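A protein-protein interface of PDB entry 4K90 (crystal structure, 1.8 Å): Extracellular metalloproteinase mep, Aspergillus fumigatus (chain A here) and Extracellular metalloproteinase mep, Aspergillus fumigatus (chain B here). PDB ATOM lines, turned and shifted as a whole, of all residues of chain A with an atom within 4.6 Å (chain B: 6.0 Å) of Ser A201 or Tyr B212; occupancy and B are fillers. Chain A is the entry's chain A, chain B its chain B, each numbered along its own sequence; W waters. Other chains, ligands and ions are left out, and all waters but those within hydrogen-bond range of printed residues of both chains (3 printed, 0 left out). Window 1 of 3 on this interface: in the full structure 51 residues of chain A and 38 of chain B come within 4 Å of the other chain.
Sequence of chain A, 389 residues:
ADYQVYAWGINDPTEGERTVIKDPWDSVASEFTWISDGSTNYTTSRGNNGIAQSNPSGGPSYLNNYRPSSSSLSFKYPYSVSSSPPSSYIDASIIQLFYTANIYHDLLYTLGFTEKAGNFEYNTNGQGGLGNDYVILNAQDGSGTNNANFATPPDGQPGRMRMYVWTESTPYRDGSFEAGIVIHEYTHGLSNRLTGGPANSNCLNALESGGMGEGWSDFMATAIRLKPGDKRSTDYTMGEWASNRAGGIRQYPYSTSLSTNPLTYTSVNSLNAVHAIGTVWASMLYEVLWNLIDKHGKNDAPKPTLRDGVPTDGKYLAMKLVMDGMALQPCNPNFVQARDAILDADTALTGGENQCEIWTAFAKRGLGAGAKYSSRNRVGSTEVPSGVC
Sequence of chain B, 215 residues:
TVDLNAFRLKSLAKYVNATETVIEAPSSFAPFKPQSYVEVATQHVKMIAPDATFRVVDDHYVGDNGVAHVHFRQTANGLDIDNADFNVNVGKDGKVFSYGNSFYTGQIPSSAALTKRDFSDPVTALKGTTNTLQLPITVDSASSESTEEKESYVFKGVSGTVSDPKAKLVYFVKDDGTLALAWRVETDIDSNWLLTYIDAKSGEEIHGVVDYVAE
The backbone carbonyl oxygen (O) of Tyr B212 sits at hydrogen-bond distance from the backbone NH (N) of Thr A152, at 2.9 Å.
The backbone NH (N) of Phe A150 lies within hydrogen-bond range of the backbone carbonyl oxygen (O) of Ala B214 (2.8 Å).
The side-chain amide oxygen (OD1) of Asn A205 lies close to the backbone carbonyl oxygen (O) of Asp B211 (3.0 Å).
The side-chain carboxylate (OE2) of Glu B186 lies within hydrogen-bond range of the indole nitrogen (NE1) of Trp B193.
OG of Ser A201 sits close to O of Pro A153, at 3.2 Å.
The backbone NH of Tyr B212 is in hydrogen-bond range of the backbone carbonyl oxygen of Trp B193, 2.8 Å away.
O of Leu B195 is in hydrogen-bond range of N of Val B210.
The backbone carbonyl oxygen of Thr A152 sits at hydrogen-bond distance from the side-chain hydroxyl of Ser A201 (2.9 Å).
OD1 of Asn A200 sits at hydrogen-bond distance from N of Asn A202 (3.0 Å).
O of Tyr B212 touches O of Phe A150, 3.5 Å away.
Val B213 touches Phe A150 (CA to O, 3.5 Å).
Tyr B212 touches Ala A151.
Trp B193 touches Pro A153.
CD2 of Tyr B212 touches CA of Pro A153 (3.7 Å).
Pro A154 touches Tyr B212.
Tyr B212 touches Ser A201.
Val B210 touches Asn A202.
OD1 of Asn A202 touches CE1 of Tyr B212 (3.8 Å).
Asn A205 touches Val B210 (ND2 to CA, 3.5 Å).
Of the printed residues of chain B, Ser A201 touches Tyr B212 (3.5 Å).
Tyr B212 touches just these residues of chain A: Phe A150 (3.5 Å), Ala A151 (3.3 Å), Thr A152 (2.9 Å), Pro A153 (3.7 Å), Pro A154 (3.5 Å), Ser A201 (3.5 Å) and Asn A202 (3.8 Å).
Of the printed residues of chain A, Val B213 touches Phe A150 and Ala A151.
Of the printed residues of chain A, Ala B214 touches Phe A150.
Printed residues of chain A within 4 Å of Val B210: Asn A202 (3.7 Å) and Asn A205 (3.5 Å).
Printed residues of chain A within 4 Å of Asp B211: Asn A205.
Of the printed residues of chain A, Leu B195 touches Asn A202.
Glu B186 touches none of the printed residues of chain A.
Asn A192 touches none of the printed residues of chain B.
The nearest printed residue of chain A that does not touch Tyr B212 is Asn A205 (4.9 Å).
Of the 12 printed residues of chain A, 8 touch a printed residue of chain B.
Printed residues of chain A that touch a printed residue of chain B: Phe A150, Ala A151, Thr A152, Pro A153, Pro A154, Ser A201, Asn A202 and Asn A205.
Hydrophobic or aromatic side chains of chain A within 4 Å of the printed part of chain B: Ala A151, Pro A153 and Pro A154.
Along chain A the printed residues that touch a printed residue of chain B span positions 150 to 205.
Hydrophobic or aromatic side chains of chain B within 4 Å of the printed part of chain A: Trp B193, Leu B195, Val B210, Tyr B212, Val B213 and Ala B214.
Among the printed residues, 15 pairs touch across the chains.
Water W2 lies within hydrogen-bond range of OD1 of Asn A202 (2.8 Å), OH of Tyr B212 (2.9 Å) and N of Ser A201 (3.0 Å).
Water W3 lies within hydrogen-bond range of OG1 of Thr A152, O of Phe A150, O of Tyr B212 and ND2 of Asn A192.
Water W1 lies within hydrogen-bond range of O of Tyr B212, ND2 of Asn A192 and O of Asp B211.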
ATOM      1  N   PHE A 150     -20.211  -2.350   0.252  1.00  0.00           N
ATOM      2  CA  PHE A 150     -18.779  -2.527   0.478  1.00  0.00           C
ATOM      3  C   PHE A 150     -18.445  -2.008   1.863  1.00  0.00           C
ATOM      4  O   PHE A 150     -18.815  -0.881   2.217  1.00  0.00           O
ATOM      5  CB  PHE A 150     -17.927  -1.796  -0.585  1.00  0.00           C
ATOM      6  CG  PHE A 150     -16.462  -2.194  -0.569  1.00  0.00           C
ATOM      7  CD1 PHE A 150     -15.973  -3.127  -1.487  1.00  0.00           C
ATOM      8  CD2 PHE A 150     -15.569  -1.638   0.372  1.00  0.00           C
ATOM      9  CE1 PHE A 150     -14.635  -3.508  -1.477  1.00  0.00           C
ATOM     10  CE2 PHE A 150     -14.225  -2.025   0.406  1.00  0.00           C
ATOM     11  CZ  PHE A 150     -13.752  -2.965  -0.530  1.00  0.00           C
ATOM     12  N   ALA A 151     -17.776  -2.848   2.647  1.00  0.00           N
ATOM     13  CA  ALA A 151     -17.334  -2.495   3.996  1.00  0.00           C
ATOM     14  C   ALA A 151     -15.847  -2.178   4.008  1.00  0.00           C
ATOM     15  O   ALA A 151     -15.026  -2.965   3.507  1.00  0.00           O
ATOM     16  CB  ALA A 151     -17.643  -3.631   4.997  1.00  0.00           C
ATOM     17  N   THR A 152     -15.506  -1.024   4.583  1.00  0.00           N
ATOM     18  CA  THR A 152     -14.120  -0.581   4.644  1.00  0.00           C
ATOM     19  C   THR A 152     -13.673  -0.316   6.082  1.00  0.00           C
ATOM     20  O   THR A 152     -13.646   0.845   6.526  1.00  0.00           O
ATOM     21  CB  THR A 152     -13.830   0.654   3.753  1.00  0.00           C
ATOM     22  OG1 THR A 152     -14.368   0.455   2.446  1.00  0.00           O
ATOM     23  CG2 THR A 152     -12.308   0.874   3.623  1.00  0.00           C
ATOM     24  N   PRO A 153     -13.298  -1.388   6.814  1.00  0.00           N
ATOM     25  CA  PRO A 153     -12.660  -1.173   8.105  1.00  0.00           C
ATOM     26  C   PRO A 153     -11.241  -0.607   7.873  1.00  0.00           C
ATOM     27  O   PRO A 153     -10.798  -0.531   6.721  1.00  0.00           O
ATOM     28  CB  PRO A 153     -12.587  -2.582   8.696  1.00  0.00           C
ATOM     29  CG  PRO A 153     -12.477  -3.484   7.488  1.00  0.00           C
ATOM     30  CD  PRO A 153     -13.397  -2.832   6.478  1.00  0.00           C
ATOM     31  N   PRO A 154     -10.538  -0.196   8.943  1.00  0.00           N
ATOM     32  CA  PRO A 154      -9.205   0.372   8.748  1.00  0.00           C
ATOM     33  C   PRO A 154      -8.217  -0.652   8.186  1.00  0.00           C
ATOM     34  O   PRO A 154      -8.509  -1.858   8.160  1.00  0.00           O
ATOM     35  CB  PRO A 154      -8.781   0.796  10.165  1.00  0.00           C
ATOM     36  CG  PRO A 154     -10.082   0.908  10.927  1.00  0.00           C
ATOM     37  CD  PRO A 154     -10.925  -0.202  10.359  1.00  0.00           C
ATOM     38  N   ASN A 192     -12.243   5.512   1.276  1.00  0.00           N
ATOM     39  CA  ASN A 192     -12.209   5.434   2.740  1.00  0.00           C
ATOM     40  C   ASN A 192     -10.816   5.155   3.304  1.00  0.00           C
ATOM     41  O   ASN A 192     -10.445   5.707   4.353  1.00  0.00           O
ATOM     42  CB  ASN A 192     -13.228   4.430   3.262  1.00  0.00           C
ATOM     43  CG  ASN A 192     -14.594   5.047   3.394  1.00  0.00           C
ATOM     44  OD1 ASN A 192     -14.794   5.932   4.232  1.00  0.00           O
ATOM     45  ND2 ASN A 192     -15.529   4.633   2.533  1.00  0.00           N
ATOM     46  N   ALA A 199      -5.223   4.265   8.635  1.00  0.00           N
ATOM     47  CA  ALA A 199      -5.668   3.851   9.968  1.00  0.00           C
ATOM     48  C   ALA A 199      -7.070   4.354  10.333  1.00  0.00           C
ATOM     49  O   ALA A 199      -7.664   3.876  11.304  1.00  0.00           O
ATOM     50  CB  ALA A 199      -4.646   4.272  11.049  1.00  0.00           C
ATOM     51  N   ASN A 200      -7.609   5.291   9.557  1.00  0.00           N
ATOM     52  CA  ASN A 200      -8.871   5.933   9.948  1.00  0.00           C
ATOM     53  C   ASN A 200      -9.956   5.755   8.894  1.00  0.00           C
ATOM     54  O   ASN A 200      -9.883   6.345   7.815  1.00  0.00           O
ATOM     55  CB  ASN A 200      -8.648   7.424  10.251  1.00  0.00           C
ATOM     56  CG  ASN A 200      -9.832   8.044  10.997  1.00  0.00           C
ATOM     57  OD1 ASN A 200     -10.862   7.406  11.190  1.00  0.00           O
ATOM     58  ND2 ASN A 200      -9.673   9.284  11.436  1.00  0.00           N
ATOM     59  N   SER A 201     -10.951   4.940   9.224  1.00  0.00           N
ATOM     60  CA  SER A 201     -12.079   4.666   8.320  1.00  0.00           C
ATOM     61  C   SER A 201     -13.344   5.442   8.696  1.00  0.00           C
ATOM     62  O   SER A 201     -14.431   5.149   8.199  1.00  0.00           O
ATOM     63  CB  SER A 201     -12.371   3.169   8.254  1.00  0.00           C
ATOM     64  OG  SER A 201     -11.456   2.538   7.377  1.00  0.00           O
ATOM     65  N   ASN A 202     -13.184   6.453   9.550  1.00  0.00           N
ATOM     66  CA  ASN A 202     -14.322   7.291   9.972  1.00  0.00           C
ATOM     67  C   ASN A 202     -14.512   8.503   9.060  1.00  0.00           C
ATOM     68  O   ASN A 202     -15.396   9.346   9.319  1.00  0.00           O
ATOM     69  CB  ASN A 202     -14.109   7.821  11.399  1.00  0.00           C
ATOM     70  CG  ASN A 202     -14.256   6.751  12.466  1.00  0.00           C
ATOM     71  OD1 ASN A 202     -14.219   5.559  12.181  1.00  0.00           O
ATOM     72  ND2 ASN A 202     -14.428   7.184  13.709  1.00  0.00           N
ATOM     73  N   CYS A 203     -13.729   8.590   7.988  1.00  0.00           N
ATOM     74  CA  CYS A 203     -13.457   9.885   7.340  1.00  0.00           C
ATOM     75  C   CYS A 203     -14.282  10.250   6.109  1.00  0.00           C
ATOM     76  O   CYS A 203     -14.064  11.312   5.513  1.00  0.00           O
ATOM     77  CB  CYS A 203     -11.961  10.013   7.024  1.00  0.00           C
ATOM     78  SG  CYS A 203     -10.991  10.074   8.564  1.00  0.00           S
ATOM     79  N   ASN A 205     -17.903   9.791   6.367  1.00  0.00           N
ATOM     80  CA  ASN A 205     -19.121   9.389   7.043  1.00  0.00           C
ATOM     81  C   ASN A 205     -20.079  10.551   7.340  1.00  0.00           C
ATOM     82  O   ASN A 205     -21.268  10.341   7.534  1.00  0.00           O
ATOM     83  CB  ASN A 205     -18.807   8.524   8.272  1.00  0.00           C
ATOM     84  CG  ASN A 205     -19.357   7.090   8.110  1.00  0.00           C
ATOM     85  OD1 ASN A 205     -18.738   6.214   7.451  1.00  0.00           O
ATOM     86  ND2 ASN A 205     -20.568   6.872   8.636  1.00  0.00           N
ATOM     87  N   GLU B 186     -18.432  -0.720  19.098  1.00  0.00           N
ATOM     88  CA  GLU B 186     -18.348  -1.365  17.791  1.00  0.00           C
ATOM     89  C   GLU B 186     -19.239  -2.604  17.700  1.00  0.00           C
ATOM     90  O   GLU B 186     -19.102  -3.543  18.501  1.00  0.00           O
ATOM     91  CB  GLU B 186     -16.900  -1.731  17.433  1.00  0.00           C
ATOM     92  CG  GLU B 186     -16.776  -2.419  16.077  1.00  0.00           C
ATOM     93  CD  GLU B 186     -15.336  -2.739  15.666  1.00  0.00           C
ATOM     94  OE1 GLU B 186     -14.395  -2.444  16.427  1.00  0.00           O
ATOM     95  OE2 GLU B 186     -15.152  -3.295  14.564  1.00  0.00           O
ATOM     96  N   ASN B 192     -24.500  -3.713   8.351  1.00  0.00           N
ATOM     97  CA  ASN B 192     -23.940  -2.459   8.840  1.00  0.00           C
ATOM     98  C   ASN B 192     -22.825  -2.826   9.785  1.00  0.00           C
ATOM     99  O   ASN B 192     -22.877  -3.866  10.422  1.00  0.00           O
ATOM    100  CB  ASN B 192     -24.990  -1.651   9.610  1.00  0.00           C
ATOM    101  CG  ASN B 192     -26.236  -1.385   8.801  1.00  0.00           C
ATOM    102  OD1 ASN B 192     -26.350  -0.351   8.140  1.00  0.00           O
ATOM    103  ND2 ASN B 192     -27.171  -2.310   8.840  1.00  0.00           N
ATOM    104  N   TRP B 193     -21.828  -1.963   9.900  1.00  0.00           N
ATOM    105  CA  TRP B 193     -20.714  -2.218  10.795  1.00  0.00           C
ATOM    106  C   TRP B 193     -20.438  -0.910  11.497  1.00  0.00           C
ATOM    107  O   TRP B 193     -19.837  -0.007  10.917  1.00  0.00           O
ATOM    108  CB  TRP B 193     -19.502  -2.663   9.977  1.00  0.00           C
ATOM    109  CG  TRP B 193     -18.271  -3.082  10.747  1.00  0.00           C
ATOM    110  CD1 TRP B 193     -17.944  -2.788  12.044  1.00  0.00           C
ATOM    111  CD2 TRP B 193     -17.177  -3.834  10.217  1.00  0.00           C
ATOM    112  NE1 TRP B 193     -16.716  -3.348  12.363  1.00  0.00           N
ATOM    113  CE2 TRP B 193     -16.229  -3.993  11.254  1.00  0.00           C
ATOM    114  CE3 TRP B 193     -16.915  -4.405   8.964  1.00  0.00           C
ATOM    115  CZ2 TRP B 193     -15.025  -4.689  11.069  1.00  0.00           C
ATOM    116  CZ3 TRP B 193     -15.721  -5.098   8.783  1.00  0.00           C
ATOM    117  CH2 TRP B 193     -14.797  -5.233   9.833  1.00  0.00           C
ATOM    118  N   LEU B 194     -20.873  -0.818  12.748  1.00  0.00           N
ATOM    119  CA  LEU B 194     -21.082   0.483  13.367  1.00  0.00           C
ATOM    120  C   LEU B 194     -20.052   0.787  14.427  1.00  0.00           C
ATOM    121  O   LEU B 194     -19.652  -0.101  15.180  1.00  0.00           O
ATOM    122  CB  LEU B 194     -22.497   0.562  13.977  1.00  0.00           C
ATOM    123  CG  LEU B 194     -23.715   0.297  13.080  1.00  0.00           C
ATOM    124  CD1 LEU B 194     -25.050   0.548  13.838  1.00  0.00           C
ATOM    125  CD2 LEU B 194     -23.629   1.130  11.815  1.00  0.00           C
ATOM    126  N   LEU B 195     -19.583   2.033  14.446  1.00  0.00           N
ATOM    127  CA  LEU B 195     -18.954   2.610  15.632  1.00  0.00           C
ATOM    128  C   LEU B 195     -19.930   3.635  16.206  1.00  0.00           C
ATOM    129  O   LEU B 195     -20.221   4.655  15.563  1.00  0.00           O
ATOM    130  CB  LEU B 195     -17.623   3.295  15.289  1.00  0.00           C
ATOM    131  CG  LEU B 195     -16.537   2.473  14.587  1.00  0.00           C
ATOM    132  CD1 LEU B 195     -15.301   3.315  14.376  1.00  0.00           C
ATOM    133  CD2 LEU B 195     -16.216   1.211  15.367  1.00  0.00           C
ATOM    134  N   VAL B 210     -20.798   5.910  13.107  1.00  0.00           N
ATOM    135  CA  VAL B 210     -20.034   5.683  11.872  1.00  0.00           C
ATOM    136  C   VAL B 210     -20.408   4.309  11.331  1.00  0.00           C
ATOM    137  O   VAL B 210     -20.445   3.354  12.098  1.00  0.00           O
ATOM    138  CB  VAL B 210     -18.517   5.730  12.169  1.00  0.00           C
ATOM    139  CG1 VAL B 210     -17.678   5.079  11.045  1.00  0.00           C
ATOM    140  CG2 VAL B 210     -18.077   7.173  12.437  1.00  0.00           C
ATOM    141  N   ASP B 211     -20.700   4.209  10.031  1.00  0.00           N
ATOM    142  CA  ASP B 211     -20.958   2.901   9.408  1.00  0.00           C
ATOM    143  C   ASP B 211     -19.835   2.611   8.408  1.00  0.00           C
ATOM    144  O   ASP B 211     -19.624   3.371   7.464  1.00  0.00           O
ATOM    145  CB  ASP B 211     -22.330   2.900   8.726  1.00  0.00           C
ATOM    146  CG  ASP B 211     -22.841   1.502   8.390  1.00  0.00           C
ATOM    147  OD1 ASP B 211     -22.069   0.525   8.411  1.00  0.00           O
ATOM    148  OD2 ASP B 211     -24.051   1.390   8.106  1.00  0.00           O
ATOM    149  N   TYR B 212     -19.105   1.522   8.631  1.00  0.00           N
ATOM    150  CA  TYR B 212     -18.080   1.082   7.673  1.00  0.00           C
ATOM    151  C   TYR B 212     -18.656   0.518   6.361  1.00  0.00           C
ATOM    152  O   TYR B 212     -17.940   0.421   5.354  1.00  0.00           O
ATOM    153  CB  TYR B 212     -17.199   0.016   8.311  1.00  0.00           C
ATOM    154  CG  TYR B 212     -16.226   0.457   9.366  1.00  0.00           C
ATOM    155  CD1 TYR B 212     -15.826   1.793   9.501  1.00  0.00           C
ATOM    156  CD2 TYR B 212     -15.634  -0.499  10.199  1.00  0.00           C
ATOM    157  CE1 TYR B 212     -14.881   2.167  10.496  1.00  0.00           C
ATOM    158  CE2 TYR B 212     -14.694  -0.156  11.161  1.00  0.00           C
ATOM    159  CZ  TYR B 212     -14.321   1.177  11.309  1.00  0.00           C
ATOM    160  OH  TYR B 212     -13.367   1.478  12.248  1.00  0.00           O
ATOM    161  N   VAL B 213     -19.947   0.180   6.365  1.00  0.00           N
ATOM    162  CA  VAL B 213     -20.614  -0.325   5.156  1.00  0.00           C
ATOM    163  C   VAL B 213     -21.226   0.828   4.376  1.00  0.00           C
ATOM    164  O   VAL B 213     -22.013   1.621   4.933  1.00  0.00           O
ATOM    165  CB  VAL B 213     -21.725  -1.348   5.489  1.00  0.00           C
ATOM    166  CG1 VAL B 213     -22.419  -1.854   4.186  1.00  0.00           C
ATOM    167  CG2 VAL B 213     -21.155  -2.517   6.289  1.00  0.00           C
ATOM    168  N   ALA B 214     -20.858   0.915   3.095  1.00  0.00           N
ATOM    169  CA  ALA B 214     -21.452   1.859   2.162  1.00  0.00           C
ATOM    170  C   ALA B 214     -22.154   1.069   1.057  1.00  0.00           C
ATOM    171  O   ALA B 214     -21.730  -0.049   0.712  1.00  0.00           O
ATOM    172  CB  ALA B 214     -20.378   2.738   1.551  1.00  0.00           C
HETATM  173  O   HOH W   1     -17.614   3.389   4.671  1.00  0.00           O
HETATM  174  O   HOH W   2     -11.991   3.967  11.844  1.00  0.00           O
HETATM  175  O   HOH W   3     -17.012   1.470   2.539  1.00  0.00           O
